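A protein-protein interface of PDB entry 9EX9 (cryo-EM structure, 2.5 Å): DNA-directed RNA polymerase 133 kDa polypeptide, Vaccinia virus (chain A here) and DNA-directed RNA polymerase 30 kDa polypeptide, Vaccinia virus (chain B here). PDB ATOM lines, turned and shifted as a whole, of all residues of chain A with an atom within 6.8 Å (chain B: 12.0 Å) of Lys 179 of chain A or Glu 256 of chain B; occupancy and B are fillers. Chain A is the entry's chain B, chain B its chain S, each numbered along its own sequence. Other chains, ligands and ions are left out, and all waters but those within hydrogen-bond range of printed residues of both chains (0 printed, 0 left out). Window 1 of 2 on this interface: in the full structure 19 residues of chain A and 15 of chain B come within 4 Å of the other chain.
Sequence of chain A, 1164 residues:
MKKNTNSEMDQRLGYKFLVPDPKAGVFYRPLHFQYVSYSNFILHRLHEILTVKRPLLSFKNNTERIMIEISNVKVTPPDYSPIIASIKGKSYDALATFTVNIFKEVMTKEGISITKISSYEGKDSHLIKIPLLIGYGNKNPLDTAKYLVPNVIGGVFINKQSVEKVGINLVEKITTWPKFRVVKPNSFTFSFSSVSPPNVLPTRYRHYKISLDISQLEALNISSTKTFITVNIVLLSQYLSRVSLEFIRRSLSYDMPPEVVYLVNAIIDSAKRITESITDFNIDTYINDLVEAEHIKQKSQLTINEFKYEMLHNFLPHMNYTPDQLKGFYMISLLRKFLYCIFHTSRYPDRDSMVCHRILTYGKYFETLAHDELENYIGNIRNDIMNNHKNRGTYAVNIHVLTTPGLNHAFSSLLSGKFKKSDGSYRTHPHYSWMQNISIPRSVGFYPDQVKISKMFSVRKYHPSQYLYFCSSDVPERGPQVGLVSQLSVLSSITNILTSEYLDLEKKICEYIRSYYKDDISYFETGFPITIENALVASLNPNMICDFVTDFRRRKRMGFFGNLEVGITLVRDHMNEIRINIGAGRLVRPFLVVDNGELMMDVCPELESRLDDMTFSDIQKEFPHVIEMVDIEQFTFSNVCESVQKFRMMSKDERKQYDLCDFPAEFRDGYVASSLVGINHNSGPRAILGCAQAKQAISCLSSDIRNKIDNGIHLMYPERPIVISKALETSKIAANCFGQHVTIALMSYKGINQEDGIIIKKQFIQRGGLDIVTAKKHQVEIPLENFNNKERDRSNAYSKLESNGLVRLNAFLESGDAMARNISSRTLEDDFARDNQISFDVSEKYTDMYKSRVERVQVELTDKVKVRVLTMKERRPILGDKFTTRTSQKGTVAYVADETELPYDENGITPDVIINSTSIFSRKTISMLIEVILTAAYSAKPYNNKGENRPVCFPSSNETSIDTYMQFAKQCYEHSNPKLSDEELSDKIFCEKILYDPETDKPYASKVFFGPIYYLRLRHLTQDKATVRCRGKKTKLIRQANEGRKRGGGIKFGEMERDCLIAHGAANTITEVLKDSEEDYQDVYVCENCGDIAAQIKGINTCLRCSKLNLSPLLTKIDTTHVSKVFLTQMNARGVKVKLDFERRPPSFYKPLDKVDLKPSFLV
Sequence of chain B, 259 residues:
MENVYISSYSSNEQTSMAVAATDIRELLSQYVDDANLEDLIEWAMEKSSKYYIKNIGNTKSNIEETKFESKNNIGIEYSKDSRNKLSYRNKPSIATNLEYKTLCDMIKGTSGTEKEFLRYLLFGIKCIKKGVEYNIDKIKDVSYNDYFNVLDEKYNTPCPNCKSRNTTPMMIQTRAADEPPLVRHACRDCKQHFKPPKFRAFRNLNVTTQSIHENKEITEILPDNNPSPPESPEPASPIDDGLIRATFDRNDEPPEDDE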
ATOM      1  N   LYS A 173      -7.440 -24.343 -18.522  1.00  0.00           N
ATOM      2  CA  LYS A 173      -8.572 -23.671 -19.148  1.00  0.00           C
ATOM      3  C   LYS A 173      -9.906 -24.119 -18.568  1.00  0.00           C
ATOM      4  O   LYS A 173     -10.905 -23.406 -18.708  1.00  0.00           O
ATOM      5  CB  LYS A 173      -8.558 -23.918 -20.656  1.00  0.00           C
ATOM      6  CG  LYS A 173      -7.311 -23.409 -21.362  1.00  0.00           C
ATOM      7  CD  LYS A 173      -7.229 -21.890 -21.376  1.00  0.00           C
ATOM      8  CE  LYS A 173      -8.309 -21.268 -22.241  1.00  0.00           C
ATOM      9  NZ  LYS A 173      -8.120 -19.800 -22.390  1.00  0.00           N
ATOM     10  N   ILE A 174      -9.952 -25.282 -17.932  1.00  0.00           N
ATOM     11  CA  ILE A 174     -11.189 -25.820 -17.382  1.00  0.00           C
ATOM     12  C   ILE A 174     -11.313 -25.383 -15.929  1.00  0.00           C
ATOM     13  O   ILE A 174     -10.433 -25.667 -15.108  1.00  0.00           O
ATOM     14  CB  ILE A 174     -11.224 -27.351 -17.511  1.00  0.00           C
ATOM     15  CG1 ILE A 174     -11.662 -27.739 -18.926  1.00  0.00           C
ATOM     16  CG2 ILE A 174     -12.147 -27.962 -16.466  1.00  0.00           C
ATOM     17  CD1 ILE A 174     -11.671 -29.223 -19.184  1.00  0.00           C
ATOM     18  N   THR A 175     -12.407 -24.699 -15.613  1.00  0.00           N
ATOM     19  CA  THR A 175     -12.669 -24.213 -14.267  1.00  0.00           C
ATOM     20  C   THR A 175     -13.446 -25.250 -13.470  1.00  0.00           C
ATOM     21  O   THR A 175     -13.901 -26.264 -14.000  1.00  0.00           O
ATOM     22  CB  THR A 175     -13.451 -22.904 -14.306  1.00  0.00           C
ATOM     23  OG1 THR A 175     -14.641 -23.080 -15.080  1.00  0.00           O
ATOM     24  CG2 THR A 175     -12.617 -21.805 -14.920  1.00  0.00           C
ATOM     25  N   TRP A 177     -16.012 -24.157 -11.198  1.00  0.00           N
ATOM     26  CA  TRP A 177     -17.324 -23.595 -10.933  1.00  0.00           C
ATOM     27  C   TRP A 177     -17.954 -23.188 -12.256  1.00  0.00           C
ATOM     28  O   TRP A 177     -17.244 -22.759 -13.168  1.00  0.00           O
ATOM     29  CB  TRP A 177     -17.248 -22.360 -10.021  1.00  0.00           C
ATOM     30  CG  TRP A 177     -16.892 -22.619  -8.582  1.00  0.00           C
ATOM     31  CD1 TRP A 177     -15.703 -23.064  -8.100  1.00  0.00           C
ATOM     32  CD2 TRP A 177     -17.731 -22.410  -7.441  1.00  0.00           C
ATOM     33  NE1 TRP A 177     -15.749 -23.161  -6.735  1.00  0.00           N
ATOM     34  CE2 TRP A 177     -16.986 -22.766  -6.306  1.00  0.00           C
ATOM     35  CE3 TRP A 177     -19.042 -21.966  -7.270  1.00  0.00           C
ATOM     36  CZ2 TRP A 177     -17.506 -22.690  -5.022  1.00  0.00           C
ATOM     37  CZ3 TRP A 177     -19.555 -21.895  -5.995  1.00  0.00           C
ATOM     38  CH2 TRP A 177     -18.790 -22.252  -4.888  1.00  0.00           C
ATOM     39  N   PRO A 178     -19.273 -23.300 -12.392  1.00  0.00           N
ATOM     40  CA  PRO A 178     -19.907 -22.867 -13.641  1.00  0.00           C
ATOM     41  C   PRO A 178     -19.729 -21.375 -13.871  1.00  0.00           C
ATOM     42  O   PRO A 178     -19.693 -20.580 -12.933  1.00  0.00           O
ATOM     43  CB  PRO A 178     -21.379 -23.228 -13.436  1.00  0.00           C
ATOM     44  CG  PRO A 178     -21.382 -24.251 -12.388  1.00  0.00           C
ATOM     45  CD  PRO A 178     -20.235 -23.949 -11.492  1.00  0.00           C
ATOM     46  N   LYS A 179     -19.632 -21.003 -15.142  1.00  0.00           N
ATOM     47  CA  LYS A 179     -19.422 -19.619 -15.546  1.00  0.00           C
ATOM     48  C   LYS A 179     -20.754 -18.965 -15.870  1.00  0.00           C
ATOM     49  O   LYS A 179     -21.542 -19.504 -16.651  1.00  0.00           O
ATOM     50  CB  LYS A 179     -18.503 -19.533 -16.762  1.00  0.00           C
ATOM     51  CG  LYS A 179     -17.075 -19.911 -16.483  1.00  0.00           C
ATOM     52  CD  LYS A 179     -16.214 -19.708 -17.710  1.00  0.00           C
ATOM     53  CE  LYS A 179     -14.781 -20.134 -17.457  1.00  0.00           C
ATOM     54  NZ  LYS A 179     -13.921 -19.956 -18.655  1.00  0.00           N
ATOM     55  N   PHE A 180     -20.992 -17.799 -15.283  1.00  0.00           N
ATOM     56  CA  PHE A 180     -22.199 -17.024 -15.515  1.00  0.00           C
ATOM     57  C   PHE A 180     -21.898 -15.903 -16.496  1.00  0.00           C
ATOM     58  O   PHE A 180     -20.783 -15.377 -16.528  1.00  0.00           O
ATOM     59  CB  PHE A 180     -22.726 -16.449 -14.202  1.00  0.00           C
ATOM     60  CG  PHE A 180     -23.887 -15.515 -14.369  1.00  0.00           C
ATOM     61  CD1 PHE A 180     -25.171 -16.001 -14.476  1.00  0.00           C
ATOM     62  CD2 PHE A 180     -23.693 -14.151 -14.405  1.00  0.00           C
ATOM     63  CE1 PHE A 180     -26.231 -15.146 -14.624  1.00  0.00           C
ATOM     64  CE2 PHE A 180     -24.753 -13.296 -14.554  1.00  0.00           C
ATOM     65  CZ  PHE A 180     -26.021 -13.793 -14.661  1.00  0.00           C
ATOM     66  N   ARG A 181     -22.889 -15.550 -17.307  1.00  0.00           N
ATOM     67  CA  ARG A 181     -22.718 -14.486 -18.281  1.00  0.00           C
ATOM     68  C   ARG A 181     -24.077 -13.911 -18.642  1.00  0.00           C
ATOM     69  O   ARG A 181     -25.049 -14.649 -18.807  1.00  0.00           O
ATOM     70  CB  ARG A 181     -22.005 -14.995 -19.534  1.00  0.00           C
ATOM     71  CG  ARG A 181     -21.926 -13.974 -20.642  1.00  0.00           C
ATOM     72  CD  ARG A 181     -21.040 -14.444 -21.777  1.00  0.00           C
ATOM     73  NE  ARG A 181     -21.045 -13.498 -22.886  1.00  0.00           N
ATOM     74  CZ  ARG A 181     -21.888 -13.538 -23.909  1.00  0.00           C
ATOM     75  NH1 ARG A 181     -22.809 -14.481 -24.013  1.00  0.00           N
ATOM     76  NH2 ARG A 181     -21.805 -12.607 -24.854  1.00  0.00           N
ATOM     77  N   THR A 189     -26.911 -16.994 -19.278  1.00  0.00           N
ATOM     78  CA  THR A 189     -26.375 -18.303 -19.619  1.00  0.00           C
ATOM     79  C   THR A 189     -25.446 -18.783 -18.512  1.00  0.00           C
ATOM     80  O   THR A 189     -24.897 -17.991 -17.748  1.00  0.00           O
ATOM     81  CB  THR A 189     -25.624 -18.271 -20.950  1.00  0.00           C
ATOM     82  OG1 THR A 189     -25.233 -19.598 -21.307  1.00  0.00           O
ATOM     83  CG2 THR A 189     -24.391 -17.411 -20.844  1.00  0.00           C
ATOM     84  N   PHE A 190     -25.264 -20.102 -18.450  1.00  0.00           N
ATOM     85  CA  PHE A 190     -24.570 -20.748 -17.335  1.00  0.00           C
ATOM     86  C   PHE A 190     -23.897 -22.000 -17.895  1.00  0.00           C
ATOM     87  O   PHE A 190     -24.573 -22.995 -18.153  1.00  0.00           O
ATOM     88  CB  PHE A 190     -25.570 -21.086 -16.239  1.00  0.00           C
ATOM     89  CG  PHE A 190     -24.995 -21.149 -14.855  1.00  0.00           C
ATOM     90  CD1 PHE A 190     -24.373 -20.054 -14.290  1.00  0.00           C
ATOM     91  CD2 PHE A 190     -25.139 -22.288 -14.093  1.00  0.00           C
ATOM     92  CE1 PHE A 190     -23.872 -20.111 -13.010  1.00  0.00           C
ATOM     93  CE2 PHE A 190     -24.643 -22.345 -12.816  1.00  0.00           C
ATOM     94  CZ  PHE A 190     -24.013 -21.254 -12.273  1.00  0.00           C
ATOM     95  N   SER A 191     -22.585 -21.949 -18.094  1.00  0.00           N
ATOM     96  CA  SER A 191     -21.870 -23.006 -18.798  1.00  0.00           C
ATOM     97  C   SER A 191     -20.895 -23.718 -17.870  1.00  0.00           C
ATOM     98  O   SER A 191     -20.227 -23.081 -17.053  1.00  0.00           O
ATOM     99  CB  SER A 191     -21.121 -22.438 -19.998  1.00  0.00           C
ATOM    100  OG  SER A 191     -20.210 -21.440 -19.595  1.00  0.00           O
ATOM    101  N   PHE A 192     -20.808 -25.040 -18.009  1.00  0.00           N
ATOM    102  CA  PHE A 192     -19.929 -25.843 -17.167  1.00  0.00           C
ATOM    103  C   PHE A 192     -19.369 -27.010 -17.976  1.00  0.00           C
ATOM    104  O   PHE A 192     -19.703 -27.194 -19.150  1.00  0.00           O
ATOM    105  CB  PHE A 192     -20.664 -26.329 -15.920  1.00  0.00           C
ATOM    106  CG  PHE A 192     -21.809 -27.244 -16.207  1.00  0.00           C
ATOM    107  CD1 PHE A 192     -22.990 -26.754 -16.721  1.00  0.00           C
ATOM    108  CD2 PHE A 192     -21.712 -28.595 -15.939  1.00  0.00           C
ATOM    109  CE1 PHE A 192     -24.047 -27.592 -16.976  1.00  0.00           C
ATOM    110  CE2 PHE A 192     -22.767 -29.438 -16.193  1.00  0.00           C
ATOM    111  CZ  PHE A 192     -23.935 -28.936 -16.712  1.00  0.00           C
ATOM    112  N   PHE A 338     -27.584 -21.271 -10.299  1.00  0.00           N
ATOM    113  CA  PHE A 338     -27.823 -20.382 -11.430  1.00  0.00           C
ATOM    114  C   PHE A 338     -28.779 -19.266 -11.042  1.00  0.00           C
ATOM    115  O   PHE A 338     -28.509 -18.085 -11.285  1.00  0.00           O
ATOM    116  CB  PHE A 338     -28.379 -21.188 -12.603  1.00  0.00           C
ATOM    117  CG  PHE A 338     -28.518 -20.412 -13.883  1.00  0.00           C
ATOM    118  CD1 PHE A 338     -27.889 -19.199 -14.066  1.00  0.00           C
ATOM    119  CD2 PHE A 338     -29.287 -20.911 -14.909  1.00  0.00           C
ATOM    120  CE1 PHE A 338     -28.027 -18.510 -15.247  1.00  0.00           C
ATOM    121  CE2 PHE A 338     -29.423 -20.222 -16.083  1.00  0.00           C
ATOM    122  CZ  PHE A 338     -28.794 -19.023 -16.251  1.00  0.00           C
ATOM    123  N   TYR A 348     -21.267 -14.289  -5.989  1.00  0.00           N
ATOM    124  CA  TYR A 348     -20.937 -15.562  -6.611  1.00  0.00           C
ATOM    125  C   TYR A 348     -19.525 -15.518  -7.188  1.00  0.00           C
ATOM    126  O   TYR A 348     -19.151 -14.525  -7.814  1.00  0.00           O
ATOM    127  CB  TYR A 348     -21.938 -15.879  -7.721  1.00  0.00           C
ATOM    128  CG  TYR A 348     -21.733 -17.218  -8.377  1.00  0.00           C
ATOM    129  CD1 TYR A 348     -22.164 -18.384  -7.767  1.00  0.00           C
ATOM    130  CD2 TYR A 348     -21.116 -17.317  -9.611  1.00  0.00           C
ATOM    131  CE1 TYR A 348     -21.976 -19.605  -8.362  1.00  0.00           C
ATOM    132  CE2 TYR A 348     -20.926 -18.534 -10.213  1.00  0.00           C
ATOM    133  CZ  TYR A 348     -21.357 -19.674  -9.584  1.00  0.00           C
ATOM    134  OH  TYR A 348     -21.170 -20.893 -10.182  1.00  0.00           O
ATOM    135  N   PRO A 349     -18.705 -16.553  -7.003  1.00  0.00           N
ATOM    136  CA  PRO A 349     -17.305 -16.474  -7.440  1.00  0.00           C
ATOM    137  C   PRO A 349     -17.156 -16.005  -8.878  1.00  0.00           C
ATOM    138  O   PRO A 349     -17.661 -16.625  -9.812  1.00  0.00           O
ATOM    139  CB  PRO A 349     -16.808 -17.909  -7.265  1.00  0.00           C
ATOM    140  CG  PRO A 349     -17.606 -18.431  -6.164  1.00  0.00           C
ATOM    141  CD  PRO A 349     -18.967 -17.812  -6.288  1.00  0.00           C
ATOM    142  N   ARG A 351     -15.335 -14.997 -12.513  1.00  0.00           N
ATOM    143  CA  ARG A 351     -14.596 -15.881 -13.407  1.00  0.00           C
ATOM    144  C   ARG A 351     -13.091 -15.697 -13.274  1.00  0.00           C
ATOM    145  O   ARG A 351     -12.332 -16.637 -13.531  1.00  0.00           O
ATOM    146  CB  ARG A 351     -15.029 -15.658 -14.855  1.00  0.00           C
ATOM    147  CG  ARG A 351     -14.679 -14.301 -15.423  1.00  0.00           C
ATOM    148  CD  ARG A 351     -14.952 -14.248 -16.916  1.00  0.00           C
ATOM    149  NE  ARG A 351     -14.531 -12.982 -17.502  1.00  0.00           N
ATOM    150  CZ  ARG A 351     -15.295 -11.901 -17.597  1.00  0.00           C
ATOM    151  NH1 ARG A 351     -16.543 -11.894 -17.158  1.00  0.00           N
ATOM    152  NH2 ARG A 351     -14.792 -10.799 -18.144  1.00  0.00           N
ATOM    153  N   HIS A 357      -9.936 -22.218 -10.186  1.00  0.00           N
ATOM    154  CA  HIS A 357      -8.867 -22.471 -11.139  1.00  0.00           C
ATOM    155  C   HIS A 357      -7.870 -23.453 -10.548  1.00  0.00           C
ATOM    156  O   HIS A 357      -7.788 -23.636  -9.332  1.00  0.00           O
ATOM    157  CB  HIS A 357      -8.150 -21.179 -11.534  1.00  0.00           C
ATOM    158  CG  HIS A 357      -8.857 -20.405 -12.597  1.00  0.00           C
ATOM    159  ND1 HIS A 357      -9.186 -19.076 -12.455  1.00  0.00           N
ATOM    160  CD2 HIS A 357      -9.300 -20.774 -13.820  1.00  0.00           C
ATOM    161  CE1 HIS A 357      -9.803 -18.659 -13.545  1.00  0.00           C
ATOM    162  NE2 HIS A 357      -9.886 -19.671 -14.388  1.00  0.00           N
ATOM    163  N   LYS A 421      -2.414 -23.181 -27.243  1.00  0.00           N
ATOM    164  CA  LYS A 421      -2.550 -21.779 -27.611  1.00  0.00           C
ATOM    165  C   LYS A 421      -1.699 -20.853 -26.752  1.00  0.00           C
ATOM    166  O   LYS A 421      -1.814 -19.631 -26.886  1.00  0.00           O
ATOM    167  CB  LYS A 421      -4.018 -21.358 -27.524  1.00  0.00           C
ATOM    168  CG  LYS A 421      -4.928 -22.146 -28.448  1.00  0.00           C
ATOM    169  CD  LYS A 421      -6.367 -21.685 -28.332  1.00  0.00           C
ATOM    170  CE  LYS A 421      -7.290 -22.526 -29.192  1.00  0.00           C
ATOM    171  NZ  LYS A 421      -8.715 -22.142 -29.007  1.00  0.00           N
ATOM    172  N   ASN B 251     -11.728 -32.712 -28.099  1.00  0.00           N
ATOM    173  CA  ASN B 251     -12.799 -31.852 -27.599  1.00  0.00           C
ATOM    174  C   ASN B 251     -12.590 -31.539 -26.118  1.00  0.00           C
ATOM    175  O   ASN B 251     -13.510 -31.624 -25.303  1.00  0.00           O
ATOM    176  CB  ASN B 251     -14.166 -32.497 -27.835  1.00  0.00           C
ATOM    177  CG  ASN B 251     -15.315 -31.567 -27.507  1.00  0.00           C
ATOM    178  OD1 ASN B 251     -15.267 -30.375 -27.807  1.00  0.00           O
ATOM    179  ND2 ASN B 251     -16.352 -32.106 -26.881  1.00  0.00           N
ATOM    180  N   ASP B 252     -11.359 -31.173 -25.772  1.00  0.00           N
ATOM    181  CA  ASP B 252     -10.956 -31.000 -24.383  1.00  0.00           C
ATOM    182  C   ASP B 252     -10.874 -29.541 -23.958  1.00  0.00           C
ATOM    183  O   ASP B 252     -10.289 -29.249 -22.910  1.00  0.00           O
ATOM    184  CB  ASP B 252      -9.610 -31.684 -24.143  1.00  0.00           C
ATOM    185  CG  ASP B 252      -8.516 -31.148 -25.040  1.00  0.00           C
ATOM    186  OD1 ASP B 252      -8.793 -30.235 -25.842  1.00  0.00           O
ATOM    187  OD2 ASP B 252      -7.374 -31.643 -24.946  1.00  0.00           O
ATOM    188  N   GLU B 253     -11.436 -28.618 -24.736  1.00  0.00           N
ATOM    189  CA  GLU B 253     -11.461 -27.215 -24.354  1.00  0.00           C
ATOM    190  C   GLU B 253     -12.866 -26.651 -24.515  1.00  0.00           C
ATOM    191  O   GLU B 253     -13.598 -27.062 -25.423  1.00  0.00           O
ATOM    192  CB  GLU B 253     -10.473 -26.398 -25.195  1.00  0.00           C
ATOM    193  CG  GLU B 253      -9.018 -26.639 -24.827  1.00  0.00           C
ATOM    194  CD  GLU B 253      -8.061 -25.785 -25.631  1.00  0.00           C
ATOM    195  OE1 GLU B 253      -8.475 -25.256 -26.684  1.00  0.00           O
ATOM    196  OE2 GLU B 253      -6.895 -25.640 -25.210  1.00  0.00           O
ATOM    197  N   PRO B 254     -13.276 -25.715 -23.659  1.00  0.00           N
ATOM    198  CA  PRO B 254     -14.621 -25.167 -23.778  1.00  0.00           C
ATOM    199  C   PRO B 254     -14.786 -24.419 -25.083  1.00  0.00           C
ATOM    200  O   PRO B 254     -13.812 -23.869 -25.633  1.00  0.00           O
ATOM    201  CB  PRO B 254     -14.729 -24.226 -22.570  1.00  0.00           C
ATOM    202  CG  PRO B 254     -13.710 -24.711 -21.614  1.00  0.00           C
ATOM    203  CD  PRO B 254     -12.590 -25.223 -22.451  1.00  0.00           C
ATOM    204  N   PRO B 255     -16.005 -24.371 -25.624  1.00  0.00           N
ATOM    205  CA  PRO B 255     -16.209 -23.658 -26.895  1.00  0.00           C
ATOM    206  C   PRO B 255     -15.863 -22.181 -26.829  1.00  0.00           C
ATOM    207  O   PRO B 255     -15.453 -21.606 -27.845  1.00  0.00           O
ATOM    208  CB  PRO B 255     -17.700 -23.877 -27.183  1.00  0.00           C
ATOM    209  CG  PRO B 255     -18.307 -24.193 -25.862  1.00  0.00           C
ATOM    210  CD  PRO B 255     -17.260 -24.930 -25.096  1.00  0.00           C
ATOM    211  N   GLU B 256     -16.022 -21.546 -25.669  1.00  0.00           N
ATOM    212  CA  GLU B 256     -15.724 -20.125 -25.499  1.00  0.00           C
ATOM    213  C   GLU B 256     -16.520 -19.280 -26.497  1.00  0.00           C
ATOM    214  O   GLU B 256     -15.965 -18.574 -27.342  1.00  0.00           O
ATOM    215  CB  GLU B 256     -14.221 -19.864 -25.639  1.00  0.00           C
ATOM    216  CG  GLU B 256     -13.349 -20.687 -24.700  1.00  0.00           C
ATOM    217  CD  GLU B 256     -13.534 -20.317 -23.241  1.00  0.00           C
ATOM    218  OE1 GLU B 256     -14.348 -19.417 -22.946  1.00  0.00           O
ATOM    219  OE2 GLU B 256     -12.859 -20.928 -22.386  1.00  0.00           O
ATOM    220  N   ASP B 257     -17.840 -19.367 -26.385  1.00  0.00           N
ATOM    221  CA  ASP B 257     -18.729 -18.606 -27.254  1.00  0.00           C
ATOM    222  C   ASP B 257     -18.670 -17.123 -26.906  1.00  0.00           C
ATOM    223  O   ASP B 257     -18.344 -16.752 -25.779  1.00  0.00           O
ATOM    224  CB  ASP B 257     -20.165 -19.120 -27.139  1.00  0.00           C
ATOM    225  CG  ASP B 257     -21.110 -18.435 -28.109  1.00  0.00           C
ATOM    226  OD1 ASP B 257     -20.640 -17.610 -28.920  1.00  0.00           O
ATOM    227  OD2 ASP B 257     -22.324 -18.722 -28.062  1.00  0.00           O
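The side-chain carboxylate of Glu 253 of chain B lies within salt-bridge range of the side-chain amino group of Lys 421 of chain A, 3.9 Å away.
The side-chain carboxylate (OE2) of Glu 256 of chain B is in salt-bridge range of the side-chain amino group (NZ) of Lys 179 of chain A (3.999 Å).
N of Lys 179 of chain A lies within hydrogen-bond range of O of Ser 191 of chain A (2.9 Å).
Among the printed residues, merely in contact across the chains: Ile 174 of chain A with Asp 252 of chain B (3.97 Å).
Printed residues of chain B within 4 Å of Lys 179 of chain A: Glu 256 (3.999 Å).
Of the printed residues of chain A, Glu 256 of chain B touches Lys 179.
No residue of chain B comes within 4 Å of Lys 173 of chain A.
No residue of chain B comes within 4 Å of Thr 175 of chain A.
No residue of chain B comes within 4 Å of Pro 178 of chain A.
No residue of chain B comes within 4 Å of Phe 180 of chain A.
No residue of chain B comes within 4 Å of Thr 189 of chain A.
No residue of chain B comes within 4 Å of Phe 190 of chain A.
Ser 191 of chain A touches none of the printed residues of chain B.
Of the printed residues of chain A, Asp 252 of chain B touches Ile 174 (3.97 Å).
Of the printed residues of chain B, Lys 421 of chain A touches Glu 253.
Of the printed residues of chain A, Glu 253 of chain B touches Lys 421.
Printed residues of chain B within 4 Å of Ile 174 of chain A: Asp 252.
Pro 349 of chain A touches none of the printed residues of chain B.
Phe 192 of chain A touches none of the printed residues of chain B.
The nearest printed residue of chain B that does not touch Ile 174 of chain A is Pro 254 of chain B (4.4 Å).
Along chain B the printed residues that touch a printed residue of chain A span positions 252 to 256.
Of the 18 printed residues of chain A, 3 touch a printed residue of chain B.
Hydrophobic or aromatic side chains of chain A that line the printed part of chain B: Ile 174.
Among the printed residues, Asp or Glu carboxylates within 4 Å of a Lys or Arg side-chain nitrogen of the other chain: Lys 179 of chain A with Glu 256 of chain B (3.999 Å) and Lys 421 of chain A with Glu 253 of chain B (3.9 Å).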
